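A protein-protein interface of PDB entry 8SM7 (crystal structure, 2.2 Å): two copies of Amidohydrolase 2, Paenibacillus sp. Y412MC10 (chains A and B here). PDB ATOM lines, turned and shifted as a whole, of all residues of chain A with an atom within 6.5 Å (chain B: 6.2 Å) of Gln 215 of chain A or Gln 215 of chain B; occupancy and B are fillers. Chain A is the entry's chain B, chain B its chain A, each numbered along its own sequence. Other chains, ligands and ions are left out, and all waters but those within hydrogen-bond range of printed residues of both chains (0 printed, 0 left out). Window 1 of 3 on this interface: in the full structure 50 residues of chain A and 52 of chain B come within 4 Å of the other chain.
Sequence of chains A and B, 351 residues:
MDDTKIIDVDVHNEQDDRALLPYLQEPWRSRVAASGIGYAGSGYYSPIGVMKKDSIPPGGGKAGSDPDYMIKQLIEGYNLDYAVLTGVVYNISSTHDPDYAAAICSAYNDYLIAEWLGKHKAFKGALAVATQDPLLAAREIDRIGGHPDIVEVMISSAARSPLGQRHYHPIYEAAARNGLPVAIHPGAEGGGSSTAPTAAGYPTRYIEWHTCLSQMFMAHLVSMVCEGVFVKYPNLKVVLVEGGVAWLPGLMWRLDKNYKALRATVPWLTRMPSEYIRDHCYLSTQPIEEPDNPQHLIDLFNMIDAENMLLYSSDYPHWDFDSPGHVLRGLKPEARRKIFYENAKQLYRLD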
ATOM      1  N   PRO A 197      13.275 -25.008  19.794  1.00  0.00           N
ATOM      2  CA  PRO A 197      12.157 -24.179  19.308  1.00  0.00           C
ATOM      3  C   PRO A 197      10.827 -24.908  19.207  1.00  0.00           C
ATOM      4  O   PRO A 197       9.819 -24.264  18.912  1.00  0.00           O
ATOM      5  CB  PRO A 197      12.634 -23.726  17.925  1.00  0.00           C
ATOM      6  CG  PRO A 197      13.631 -24.768  17.489  1.00  0.00           C
ATOM      7  CD  PRO A 197      14.165 -25.463  18.709  1.00  0.00           C
ATOM      8  N   THR A 198      10.773 -26.217  19.424  1.00  0.00           N
ATOM      9  CA  THR A 198       9.491 -26.906  19.438  1.00  0.00           C
ATOM     10  C   THR A 198       9.594 -28.014  20.458  1.00  0.00           C
ATOM     11  O   THR A 198      10.694 -28.444  20.812  1.00  0.00           O
ATOM     12  CB  THR A 198       9.094 -27.522  18.079  1.00  0.00           C
ATOM     13  OG1 THR A 198       9.836 -28.738  17.871  1.00  0.00           O
ATOM     14  CG2 THR A 198       9.326 -26.553  16.910  1.00  0.00           C
ATOM     15  N   ALA A 199       8.426 -28.471  20.928  1.00  0.00           N
ATOM     16  CA  ALA A 199       8.402 -29.535  21.928  1.00  0.00           C
ATOM     17  C   ALA A 199       9.156 -30.765  21.446  1.00  0.00           C
ATOM     18  O   ALA A 199       9.744 -31.491  22.261  1.00  0.00           O
ATOM     19  CB  ALA A 199       6.962 -29.899  22.274  1.00  0.00           C
ATOM     20  N   ALA A 200       9.163 -31.011  20.130  1.00  0.00           N
ATOM     21  CA  ALA A 200       9.817 -32.182  19.564  1.00  0.00           C
ATOM     22  C   ALA A 200      11.262 -31.913  19.179  1.00  0.00           C
ATOM     23  O   ALA A 200      11.904 -32.786  18.578  1.00  0.00           O
ATOM     24  CB  ALA A 200       9.042 -32.691  18.345  1.00  0.00           C
ATOM     25  N   GLU A 208       8.581 -25.228   8.891  1.00  0.00           N
ATOM     26  CA  GLU A 208       8.240 -25.875  10.160  1.00  0.00           C
ATOM     27  C   GLU A 208       8.474 -24.945  11.348  1.00  0.00           C
ATOM     28  O   GLU A 208       7.619 -24.827  12.238  1.00  0.00           O
ATOM     29  CB  GLU A 208       9.062 -27.137  10.386  1.00  0.00           C
ATOM     30  CG  GLU A 208       9.106 -28.130   9.296  1.00  0.00           C
ATOM     31  CD  GLU A 208      10.118 -29.186   9.632  1.00  0.00           C
ATOM     32  OE1 GLU A 208       9.907 -29.909  10.643  1.00  0.00           O
ATOM     33  OE2 GLU A 208      11.141 -29.257   8.924  1.00  0.00           O
ATOM     34  N   THR A 211       5.754 -22.075  11.388  1.00  0.00           N
ATOM     35  CA  THR A 211       4.456 -22.632  11.755  1.00  0.00           C
ATOM     36  C   THR A 211       4.380 -22.943  13.249  1.00  0.00           C
ATOM     37  O   THR A 211       3.368 -22.667  13.906  1.00  0.00           O
ATOM     38  CB  THR A 211       4.194 -23.895  10.924  1.00  0.00           C
ATOM     39  OG1 THR A 211       4.208 -23.542   9.539  1.00  0.00           O
ATOM     40  CG2 THR A 211       2.838 -24.500  11.247  1.00  0.00           C
ATOM     41  N   CYS A 212       5.442 -23.504  13.808  1.00  0.00           N
ATOM     42  CA  CYS A 212       5.371 -24.003  15.172  1.00  0.00           C
ATOM     43  C   CYS A 212       5.443 -22.906  16.237  1.00  0.00           C
ATOM     44  O   CYS A 212       5.192 -23.200  17.410  1.00  0.00           O
ATOM     45  CB  CYS A 212       6.478 -25.042  15.387  1.00  0.00           C
ATOM     46  SG  CYS A 212       6.066 -26.679  14.652  1.00  0.00           S
ATOM     47  N   LEU A 213       5.746 -21.654  15.879  1.00  0.00           N
ATOM     48  CA  LEU A 213       5.972 -20.652  16.916  1.00  0.00           C
ATOM     49  C   LEU A 213       4.770 -20.519  17.850  1.00  0.00           C
ATOM     50  O   LEU A 213       4.932 -20.308  19.060  1.00  0.00           O
ATOM     51  CB  LEU A 213       6.317 -19.306  16.290  1.00  0.00           C
ATOM     52  CG  LEU A 213       7.539 -19.264  15.385  1.00  0.00           C
ATOM     53  CD1 LEU A 213       7.531 -17.966  14.603  1.00  0.00           C
ATOM     54  CD2 LEU A 213       8.813 -19.404  16.172  1.00  0.00           C
ATOM     55  N   SER A 214       3.554 -20.639  17.315  1.00  0.00           N
ATOM     56  CA  SER A 214       2.378 -20.592  18.177  1.00  0.00           C
ATOM     57  C   SER A 214       2.510 -21.527  19.369  1.00  0.00           C
ATOM     58  O   SER A 214       2.000 -21.228  20.455  1.00  0.00           O
ATOM     59  CB  SER A 214       1.133 -20.947  17.374  1.00  0.00           C
ATOM     60  OG  SER A 214       1.167 -20.265  16.130  1.00  0.00           O
ATOM     61  N   GLN A 215       3.181 -22.667  19.187  1.00  0.00           N
ATOM     62  CA  GLN A 215       3.226 -23.658  20.253  1.00  0.00           C
ATOM     63  C   GLN A 215       4.088 -23.191  21.408  1.00  0.00           C
ATOM     64  O   GLN A 215       3.835 -23.561  22.568  1.00  0.00           O
ATOM     65  CB  GLN A 215       3.725 -24.984  19.706  1.00  0.00           C
ATOM     66  CG  GLN A 215       2.758 -25.591  18.718  1.00  0.00           C
ATOM     67  CD  GLN A 215       3.475 -26.435  17.684  1.00  0.00           C
ATOM     68  OE1 GLN A 215       4.370 -27.203  18.022  1.00  0.00           O
ATOM     69  NE2 GLN A 215       3.091 -26.297  16.426  1.00  0.00           N
ATOM     70  N   MET A 216       5.088 -22.364  21.114  1.00  0.00           N
ATOM     71  CA  MET A 216       5.857 -21.734  22.175  1.00  0.00           C
ATOM     72  C   MET A 216       4.971 -20.829  23.034  1.00  0.00           C
ATOM     73  O   MET A 216       5.053 -20.862  24.268  1.00  0.00           O
ATOM     74  CB  MET A 216       7.031 -20.966  21.565  1.00  0.00           C
ATOM     75  CG  MET A 216       7.988 -20.395  22.589  1.00  0.00           C
ATOM     76  SD  MET A 216       9.094 -21.672  23.232  1.00  0.00           S
ATOM     77  CE  MET A 216      10.131 -22.001  21.789  1.00  0.00           C
ATOM     78  N   PHE A 217       4.102 -20.028  22.397  1.00  0.00           N
ATOM     79  CA  PHE A 217       3.187 -19.167  23.145  1.00  0.00           C
ATOM     80  C   PHE A 217       2.243 -19.985  24.007  1.00  0.00           C
ATOM     81  O   PHE A 217       1.939 -19.599  25.139  1.00  0.00           O
ATOM     82  CB  PHE A 217       2.362 -18.292  22.206  1.00  0.00           C
ATOM     83  CG  PHE A 217       3.062 -17.061  21.749  1.00  0.00           C
ATOM     84  CD1 PHE A 217       4.421 -16.900  21.957  1.00  0.00           C
ATOM     85  CD2 PHE A 217       2.360 -16.059  21.095  1.00  0.00           C
ATOM     86  CE1 PHE A 217       5.081 -15.751  21.519  1.00  0.00           C
ATOM     87  CE2 PHE A 217       3.006 -14.899  20.664  1.00  0.00           C
ATOM     88  CZ  PHE A 217       4.371 -14.749  20.875  1.00  0.00           C
ATOM     89  N   MET A 218       1.738 -21.101  23.484  1.00  0.00           N
ATOM     90  CA  MET A 218       0.853 -21.918  24.307  1.00  0.00           C
ATOM     91  C   MET A 218       1.575 -22.435  25.540  1.00  0.00           C
ATOM     92  O   MET A 218       1.015 -22.430  26.642  1.00  0.00           O
ATOM     93  CB  MET A 218       0.271 -23.072  23.494  1.00  0.00           C
ATOM     94  CG  MET A 218      -0.301 -22.669  22.192  1.00  0.00           C
ATOM     95  SD  MET A 218      -0.871 -24.124  21.274  1.00  0.00           S
ATOM     96  CE  MET A 218      -0.465 -23.574  19.628  1.00  0.00           C
ATOM     97  N   ALA A 219       2.816 -22.894  25.375  1.00  0.00           N
ATOM     98  CA  ALA A 219       3.599 -23.340  26.521  1.00  0.00           C
ATOM     99  C   ALA A 219       3.806 -22.202  27.515  1.00  0.00           C
ATOM    100  O   ALA A 219       3.504 -22.342  28.707  1.00  0.00           O
ATOM    101  CB  ALA A 219       4.939 -23.905  26.058  1.00  0.00           C
ATOM    102  N   HIS A 220       4.322 -21.062  27.042  1.00  0.00           N
ATOM    103  CA  HIS A 220       4.562 -19.935  27.935  1.00  0.00           C
ATOM    104  C   HIS A 220       3.280 -19.519  28.640  1.00  0.00           C
ATOM    105  O   HIS A 220       3.292 -19.199  29.834  1.00  0.00           O
ATOM    106  CB  HIS A 220       5.141 -18.754  27.168  1.00  0.00           C
ATOM    107  CG  HIS A 220       6.593 -18.886  26.840  1.00  0.00           C
ATOM    108  ND1 HIS A 220       7.510 -19.460  27.699  1.00  0.00           N
ATOM    109  CD2 HIS A 220       7.296 -18.503  25.745  1.00  0.00           C
ATOM    110  CE1 HIS A 220       8.710 -19.435  27.146  1.00  0.00           C
ATOM    111  NE2 HIS A 220       8.608 -18.857  25.960  1.00  0.00           N
ATOM    112  N   VAL A 222       0.497 -21.321  29.296  1.00  0.00           N
ATOM    113  CA  VAL A 222       0.056 -22.269  30.310  1.00  0.00           C
ATOM    114  C   VAL A 222       0.893 -22.092  31.566  1.00  0.00           C
ATOM    115  O   VAL A 222       0.388 -22.191  32.692  1.00  0.00           O
ATOM    116  CB  VAL A 222       0.124 -23.709  29.768  1.00  0.00           C
ATOM    117  CG1 VAL A 222       0.004 -24.702  30.887  1.00  0.00           C
ATOM    118  CG2 VAL A 222      -0.959 -23.932  28.706  1.00  0.00           C
ATOM    119  N   GLY A 243       1.611 -14.539  17.158  1.00  0.00           N
ATOM    120  CA  GLY A 243       1.655 -15.967  17.417  1.00  0.00           C
ATOM    121  C   GLY A 243       0.388 -16.716  17.055  1.00  0.00           C
ATOM    122  O   GLY A 243       0.222 -17.873  17.460  1.00  0.00           O
ATOM    123  N   TRP A 247      -5.727 -21.078  17.821  1.00  0.00           N
ATOM    124  CA  TRP A 247      -5.409 -22.146  18.761  1.00  0.00           C
ATOM    125  C   TRP A 247      -5.965 -21.876  20.151  1.00  0.00           C
ATOM    126  O   TRP A 247      -5.988 -22.792  20.979  1.00  0.00           O
ATOM    127  CB  TRP A 247      -3.885 -22.347  18.844  1.00  0.00           C
ATOM    128  CG  TRP A 247      -3.122 -21.061  19.048  1.00  0.00           C
ATOM    129  CD1 TRP A 247      -2.534 -20.292  18.079  1.00  0.00           C
ATOM    130  CD2 TRP A 247      -2.870 -20.395  20.299  1.00  0.00           C
ATOM    131  NE1 TRP A 247      -1.940 -19.190  18.648  1.00  0.00           N
ATOM    132  CE2 TRP A 247      -2.133 -19.224  20.006  1.00  0.00           C
ATOM    133  CE3 TRP A 247      -3.208 -20.671  21.636  1.00  0.00           C
ATOM    134  CZ2 TRP A 247      -1.717 -18.327  20.998  1.00  0.00           C
ATOM    135  CZ3 TRP A 247      -2.791 -19.781  22.629  1.00  0.00           C
ATOM    136  CH2 TRP A 247      -2.050 -18.618  22.299  1.00  0.00           C
ATOM    137  N   LEU A 251      -6.956 -24.558  23.539  1.00  0.00           N
ATOM    138  CA  LEU A 251      -6.116 -24.466  24.727  1.00  0.00           C
ATOM    139  C   LEU A 251      -6.950 -24.092  25.947  1.00  0.00           C
ATOM    140  O   LEU A 251      -6.754 -24.627  27.043  1.00  0.00           O
ATOM    141  CB  LEU A 251      -5.007 -23.438  24.509  1.00  0.00           C
ATOM    142  CG  LEU A 251      -4.064 -23.273  25.699  1.00  0.00           C
ATOM    143  CD1 LEU A 251      -3.160 -24.474  25.744  1.00  0.00           C
ATOM    144  CD2 LEU A 251      -3.233 -22.018  25.565  1.00  0.00           C
ATOM    145  N   PRO B 197       9.679 -31.474  27.361  1.00  0.00           N
ATOM    146  CA  PRO B 197       8.280 -31.840  27.076  1.00  0.00           C
ATOM    147  C   PRO B 197       7.435 -30.738  26.479  1.00  0.00           C
ATOM    148  O   PRO B 197       6.351 -31.041  25.957  1.00  0.00           O
ATOM    149  CB  PRO B 197       7.724 -32.242  28.457  1.00  0.00           C
ATOM    150  CG  PRO B 197       8.707 -31.688  29.486  1.00  0.00           C
ATOM    151  CD  PRO B 197       9.928 -31.171  28.786  1.00  0.00           C
ATOM    152  N   THR B 198       7.847 -29.480  26.578  1.00  0.00           N
ATOM    153  CA  THR B 198       7.173 -28.373  25.911  1.00  0.00           C
ATOM    154  C   THR B 198       8.223 -27.568  25.167  1.00  0.00           C
ATOM    155  O   THR B 198       9.419 -27.677  25.442  1.00  0.00           O
ATOM    156  CB  THR B 198       6.434 -27.430  26.889  1.00  0.00           C
ATOM    157  OG1 THR B 198       7.395 -26.580  27.534  1.00  0.00           O
ATOM    158  CG2 THR B 198       5.662 -28.213  27.928  1.00  0.00           C
ATOM    159  N   ALA B 199       7.766 -26.734  24.239  1.00  0.00           N
ATOM    160  CA  ALA B 199       8.687 -25.860  23.522  1.00  0.00           C
ATOM    161  C   ALA B 199       9.401 -24.880  24.458  1.00  0.00           C
ATOM    162  O   ALA B 199      10.491 -24.388  24.127  1.00  0.00           O
ATOM    163  CB  ALA B 199       7.923 -25.099  22.438  1.00  0.00           C
ATOM    164  N   ALA B 200       8.813 -24.568  25.614  1.00  0.00           N
ATOM    165  CA  ALA B 200       9.457 -23.653  26.544  1.00  0.00           C
ATOM    166  C   ALA B 200      10.346 -24.369  27.554  1.00  0.00           C
ATOM    167  O   ALA B 200      10.901 -23.710  28.446  1.00  0.00           O
ATOM    168  CB  ALA B 200       8.408 -22.816  27.279  1.00  0.00           C
ATOM    169  N   THR B 211      -1.552 -30.471  29.961  1.00  0.00           N
ATOM    170  CA  THR B 211      -2.232 -29.566  29.035  1.00  0.00           C
ATOM    171  C   THR B 211      -1.438 -29.400  27.736  1.00  0.00           C
ATOM    172  O   THR B 211      -2.012 -29.403  26.637  1.00  0.00           O
ATOM    173  CB  THR B 211      -2.464 -28.221  29.734  1.00  0.00           C
ATOM    174  OG1 THR B 211      -3.289 -28.423  30.901  1.00  0.00           O
ATOM    175  CG2 THR B 211      -3.137 -27.225  28.791  1.00  0.00           C
ATOM    176  N   CYS B 212      -0.108 -29.313  27.847  1.00  0.00           N
ATOM    177  CA  CYS B 212       0.804 -29.033  26.756  1.00  0.00           C
ATOM    178  C   CYS B 212       1.107 -30.246  25.886  1.00  0.00           C
ATOM    179  O   CYS B 212       1.878 -30.111  24.929  1.00  0.00           O
ATOM    180  CB  CYS B 212       2.117 -28.484  27.310  1.00  0.00           C
ATOM    181  SG  CYS B 212       1.999 -26.838  27.968  1.00  0.00           S
ATOM    182  N   LEU B 213       0.543 -31.420  26.185  1.00  0.00           N
ATOM    183  CA  LEU B 213       0.843 -32.578  25.349  1.00  0.00           C
ATOM    184  C   LEU B 213       0.421 -32.342  23.897  1.00  0.00           C
ATOM    185  O   LEU B 213       1.122 -32.750  22.968  1.00  0.00           O
ATOM    186  CB  LEU B 213       0.184 -33.823  25.923  1.00  0.00           C
ATOM    187  CG  LEU B 213       0.787 -34.288  27.255  1.00  0.00           C
ATOM    188  CD1 LEU B 213      -0.059 -35.423  27.851  1.00  0.00           C
ATOM    189  CD2 LEU B 213       2.254 -34.705  27.109  1.00  0.00           C
ATOM    190  N   SER B 214      -0.708 -31.661  23.683  1.00  0.00           N
ATOM    191  CA  SER B 214      -1.161 -31.370  22.325  1.00  0.00           C
ATOM    192  C   SER B 214      -0.053 -30.759  21.493  1.00  0.00           C
ATOM    193  O   SER B 214       0.073 -31.038  20.297  1.00  0.00           O
ATOM    194  CB  SER B 214      -2.341 -30.403  22.361  1.00  0.00           C
ATOM    195  OG  SER B 214      -3.306 -30.864  23.255  1.00  0.00           O
ATOM    196  N   GLN B 215       0.746 -29.898  22.110  1.00  0.00           N
ATOM    197  CA  GLN B 215       1.775 -29.196  21.373  1.00  0.00           C
ATOM    198  C   GLN B 215       2.838 -30.151  20.845  1.00  0.00           C
ATOM    199  O   GLN B 215       3.363 -29.943  19.744  1.00  0.00           O
ATOM    200  CB  GLN B 215       2.368 -28.123  22.262  1.00  0.00           C
ATOM    201  CG  GLN B 215       1.312 -27.123  22.700  1.00  0.00           C
ATOM    202  CD  GLN B 215       1.677 -26.462  24.006  1.00  0.00           C
ATOM    203  OE1 GLN B 215       2.854 -26.162  24.261  1.00  0.00           O
ATOM    204  NE2 GLN B 215       0.675 -26.240  24.852  1.00  0.00           N
ATOM    205  N   MET B 216       3.161 -31.209  21.605  1.00  0.00           N
ATOM    206  CA  MET B 216       4.037 -32.255  21.070  1.00  0.00           C
ATOM    207  C   MET B 216       3.479 -32.859  19.782  1.00  0.00           C
ATOM    208  O   MET B 216       4.224 -33.073  18.821  1.00  0.00           O
ATOM    209  CB  MET B 216       4.242 -33.365  22.090  1.00  0.00           C
ATOM    210  CG  MET B 216       5.395 -34.284  21.746  1.00  0.00           C
ATOM    211  SD  MET B 216       7.001 -33.464  21.780  1.00  0.00           S
ATOM    212  CE  MET B 216       7.537 -33.811  23.461  1.00  0.00           C
ATOM    213  N   PHE B 217       2.177 -33.161  19.749  1.00  0.00           N
ATOM    214  CA  PHE B 217       1.571 -33.691  18.532  1.00  0.00           C
ATOM    215  C   PHE B 217       1.677 -32.680  17.402  1.00  0.00           C
ATOM    216  O   PHE B 217       2.052 -33.018  16.273  1.00  0.00           O
ATOM    217  CB  PHE B 217       0.102 -34.043  18.778  1.00  0.00           C
ATOM    218  CG  PHE B 217      -0.107 -35.412  19.331  1.00  0.00           C
ATOM    219  CD1 PHE B 217       0.932 -36.095  19.930  1.00  0.00           C
ATOM    220  CD2 PHE B 217      -1.356 -36.003  19.294  1.00  0.00           C
ATOM    221  CE1 PHE B 217       0.740 -37.365  20.473  1.00  0.00           C
ATOM    222  CE2 PHE B 217      -1.558 -37.280  19.830  1.00  0.00           C
ATOM    223  CZ  PHE B 217      -0.500 -37.960  20.408  1.00  0.00           C
ATOM    224  N   MET B 218       1.368 -31.422  17.697  1.00  0.00           N
ATOM    225  CA  MET B 218       1.435 -30.394  16.672  1.00  0.00           C
ATOM    226  C   MET B 218       2.812 -30.341  16.035  1.00  0.00           C
ATOM    227  O   MET B 218       2.931 -30.230  14.809  1.00  0.00           O
ATOM    228  CB  MET B 218       1.064 -29.043  17.276  1.00  0.00           C
ATOM    229  CG  MET B 218      -0.402 -28.937  17.621  1.00  0.00           C
ATOM    230  SD  MET B 218      -0.765 -27.334  18.334  1.00  0.00           S
ATOM    231  CE  MET B 218      -1.392 -27.807  19.957  1.00  0.00           C
ATOM    232  N   ALA B 219       3.867 -30.412  16.852  1.00  0.00           N
ATOM    233  CA  ALA B 219       5.214 -30.328  16.304  1.00  0.00           C
ATOM    234  C   ALA B 219       5.531 -31.554  15.446  1.00  0.00           C
ATOM    235  O   ALA B 219       6.018 -31.413  14.320  1.00  0.00           O
ATOM    236  CB  ALA B 219       6.237 -30.150  17.423  1.00  0.00           C
ATOM    237  N   HIS B 220       5.246 -32.761  15.946  1.00  0.00           N
ATOM    238  CA  HIS B 220       5.472 -33.963  15.137  1.00  0.00           C
ATOM    239  C   HIS B 220       4.656 -33.932  13.845  1.00  0.00           C
ATOM    240  O   HIS B 220       5.160 -34.298  12.772  1.00  0.00           O
ATOM    241  CB  HIS B 220       5.115 -35.227  15.920  1.00  0.00           C
ATOM    242  CG  HIS B 220       6.057 -35.551  17.037  1.00  0.00           C
ATOM    243  ND1 HIS B 220       7.426 -35.562  16.879  1.00  0.00           N
ATOM    244  CD2 HIS B 220       5.824 -35.914  18.322  1.00  0.00           C
ATOM    245  CE1 HIS B 220       7.998 -35.883  18.027  1.00  0.00           C
ATOM    246  NE2 HIS B 220       7.047 -36.120  18.913  1.00  0.00           N
ATOM    247  N   VAL B 222       3.500 -31.347  12.090  1.00  0.00           N
ATOM    248  CA  VAL B 222       4.081 -30.397  11.145  1.00  0.00           C
ATOM    249  C   VAL B 222       5.367 -30.960  10.562  1.00  0.00           C
ATOM    250  O   VAL B 222       5.698 -30.706   9.396  1.00  0.00           O
ATOM    251  CB  VAL B 222       4.319 -29.033  11.831  1.00  0.00           C
ATOM    252  CG1 VAL B 222       5.101 -28.113  10.931  1.00  0.00           C
ATOM    253  CG2 VAL B 222       2.981 -28.388  12.265  1.00  0.00           C
ATOM    254  N   GLY B 243      -4.485 -36.689  22.035  1.00  0.00           N
ATOM    255  CA  GLY B 243      -3.747 -35.439  22.015  1.00  0.00           C
ATOM    256  C   GLY B 243      -4.612 -34.241  21.680  1.00  0.00           C
ATOM    257  O   GLY B 243      -4.104 -33.155  21.375  1.00  0.00           O
ATOM    258  N   TRP B 247      -7.296 -28.096  18.407  1.00  0.00           N
ATOM    259  CA  TRP B 247      -6.188 -27.337  17.833  1.00  0.00           C
ATOM    260  C   TRP B 247      -5.992 -27.588  16.327  1.00  0.00           C
ATOM    261  O   TRP B 247      -5.285 -26.816  15.671  1.00  0.00           O
ATOM    262  CB  TRP B 247      -4.894 -27.651  18.597  1.00  0.00           C
ATOM    263  CG  TRP B 247      -4.629 -29.105  18.704  1.00  0.00           C
ATOM    264  CD1 TRP B 247      -4.902 -29.904  19.763  1.00  0.00           C
ATOM    265  CD2 TRP B 247      -4.066 -29.950  17.691  1.00  0.00           C
ATOM    266  NE1 TRP B 247      -4.533 -31.205  19.484  1.00  0.00           N
ATOM    267  CE2 TRP B 247      -4.027 -31.260  18.213  1.00  0.00           C
ATOM    268  CE3 TRP B 247      -3.604 -29.727  16.389  1.00  0.00           C
ATOM    269  CZ2 TRP B 247      -3.529 -32.346  17.490  1.00  0.00           C
ATOM    270  CZ3 TRP B 247      -3.111 -30.808  15.664  1.00  0.00           C
ATOM    271  CH2 TRP B 247      -3.078 -32.106  16.223  1.00  0.00           C
ATOM    272  N   LEU B 251      -4.023 -25.011  13.213  1.00  0.00           N
ATOM    273  CA  LEU B 251      -2.787 -25.541  12.643  1.00  0.00           C
ATOM    274  C   LEU B 251      -2.911 -25.715  11.127  1.00  0.00           C
ATOM    275  O   LEU B 251      -1.983 -25.377  10.376  1.00  0.00           O
ATOM    276  CB  LEU B 251      -2.419 -26.866  13.322  1.00  0.00           C
ATOM    277  CG  LEU B 251      -1.094 -27.532  12.914  1.00  0.00           C
ATOM    278  CD1 LEU B 251       0.066 -26.632  13.258  1.00  0.00           C
ATOM    279  CD2 LEU B 251      -0.913 -28.896  13.558  1.00  0.00           C
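N of Ala 200 of chain A is in hydrogen-bond range of SD of Met 216 of chain B (3.7 Å).
The backbone NH (N) of Ala 200 of chain B is in hydrogen-bond range of the side-chain sulfur (SD) of Met 216 of chain A, at 3.8 Å.
The backbone NH (N) of Ala 219 of chain B is in hydrogen-bond range of the side-chain amide oxygen (OE1) of Gln 215 of chain A (3.5 Å).
The backbone carbonyl oxygen (O) of Ala 199 of chain A lies close to the side-chain sulfur (SD) of Met 216 of chain B (3.4 Å).
The side-chain sulfur of Met 216 of chain A sits close to the backbone carbonyl oxygen of Ala 199 of chain B (3.2 Å).
OE1 of Gln 215 of chain B sits at hydrogen-bond distance from N of Ala 219 of chain A, at 3.5 Å.
The backbone carbonyl oxygen (O) of Gln 215 of chain A sits close to the side-chain amide oxygen (OE1) of Gln 215 of chain B (3.3 Å).
OG1 of Thr 198 of chain A sits close to N of Ala 200 of chain A (3.3 Å).
The side-chain hydroxyl (OG1) of Thr 198 of chain B lies close to the backbone NH (N) of Ala 200 of chain B (3.1 Å).
The backbone carbonyl oxygen of Glu 208 of chain A lies close to the side-chain sulfur of Cys 212 of chain A (3.4 Å).
SG of Cys 212 of chain B lies close to NE2 of Gln 215 of chain B, 3.4 Å away.
SG of Cys 212 of chain A lies close to NE2 of Gln 215 of chain A.
Ala 199 of chain A touches Pro 197 of chain B.
Ala 199 of chain A touches Ala 199 of chain B.
Ala 219 of chain B touches Ala 200 of chain A.
Glu 208 of chain A touches Val 222 of chain B (CA to CG1, 3.9 Å).
NE2 of Gln 215 of chain A touches CB of Met 218 of chain B, at 3.5 Å.
CB of Met 218 of chain A touches NE2 of Gln 215 of chain B, 3.5 Å away.
Thr 198 of chain B touches Ala 219 of chain A (CB to CB, 3.9 Å).
Ala 219 of chain A touches Ala 200 of chain B (CB to CB, 3.8 Å).
CE1 of His 220 of chain A touches CB of Ala 200 of chain B (3.4 Å).
Thr 211 of chain B touches Val 222 of chain A.
Gln 215 of chain A touches just these residues of chain B: Gln 215, Met 218 and Ala 219.
Gln 215 of chain B touches just these residues of chain A: Gln 215, Met 218 and Ala 219.
Printed residues of chain A within 4 Å of Thr 198 of chain B: Ala 199 (3.8 Å) and Ala 219 (3.9 Å).
Of the printed residues of chain A, Pro 197 of chain B touches Ala 199 (3.9 Å).
Of the printed residues of chain B, Ala 199 of chain A touches Pro 197 (3.9 Å), Thr 198 (3.8 Å), Ala 199 (3.7 Å) and Met 216 (3.4 Å).
Of the printed residues of chain B, Ala 200 of chain A touches Met 216 (3.7 Å), Ala 219 (3.9 Å) and His 220 (3.4 Å).
The nearest printed residue of chain B that does not touch Gln 215 of chain A is Ala 199 of chain B (4.4 Å).
The nearest residue of chain A that does not touch Gln 215 of chain B is Leu 251 of chain A (4.3 Å).
The nearest printed residue of chain B that does not touch Ala 200 of chain A is Gln 215 of chain B (5.9 Å).
Of the 19 printed residues of chain A, 10 touch a printed residue of chain B.
Hydrophobic or aromatic side chains of chain A that line the printed part of chain B: Ala 199, Ala 200, Met 216, Met 218, Ala 219, His 220 and Val 222.
Of the 18 printed residues of chain B, 11 touch a printed residue of chain A.
Printed residues of chain B that touch a printed residue of chain A: Pro 197, Thr 198, Ala 199, Ala 200, Thr 211, Gln 215, Met 216, Met 218, Ala 219, His 220 and Val 222.
Hydrophobic or aromatic side chains of chain B that line the printed part of chain A: Ala 199, Ala 200, Met 216, Met 218, Ala 219, His 220 and Val 222.
Among the printed residues, 22 pairs touch across the chains.
Ala 199 of chain A touches its own counterpart, Ala 199 of chain B.
Ala 200 of chain A touches His 220 of chain B, and with the chains exchanged His 220 of chain A touches Ala 200 of chain B.
Gln 215 of chain B touches its own counterpart, Gln 215 of chain A.
Gln 215 of chain A touches Ala 219 of chain B, and with the chains exchanged Ala 219 of chain A touches Gln 215 of chain B.
18 positions are printed for both chains.
Of the 22 pairs that touch across the chains among the printed residues, 19 have their exchanged pair printed and touching as well.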
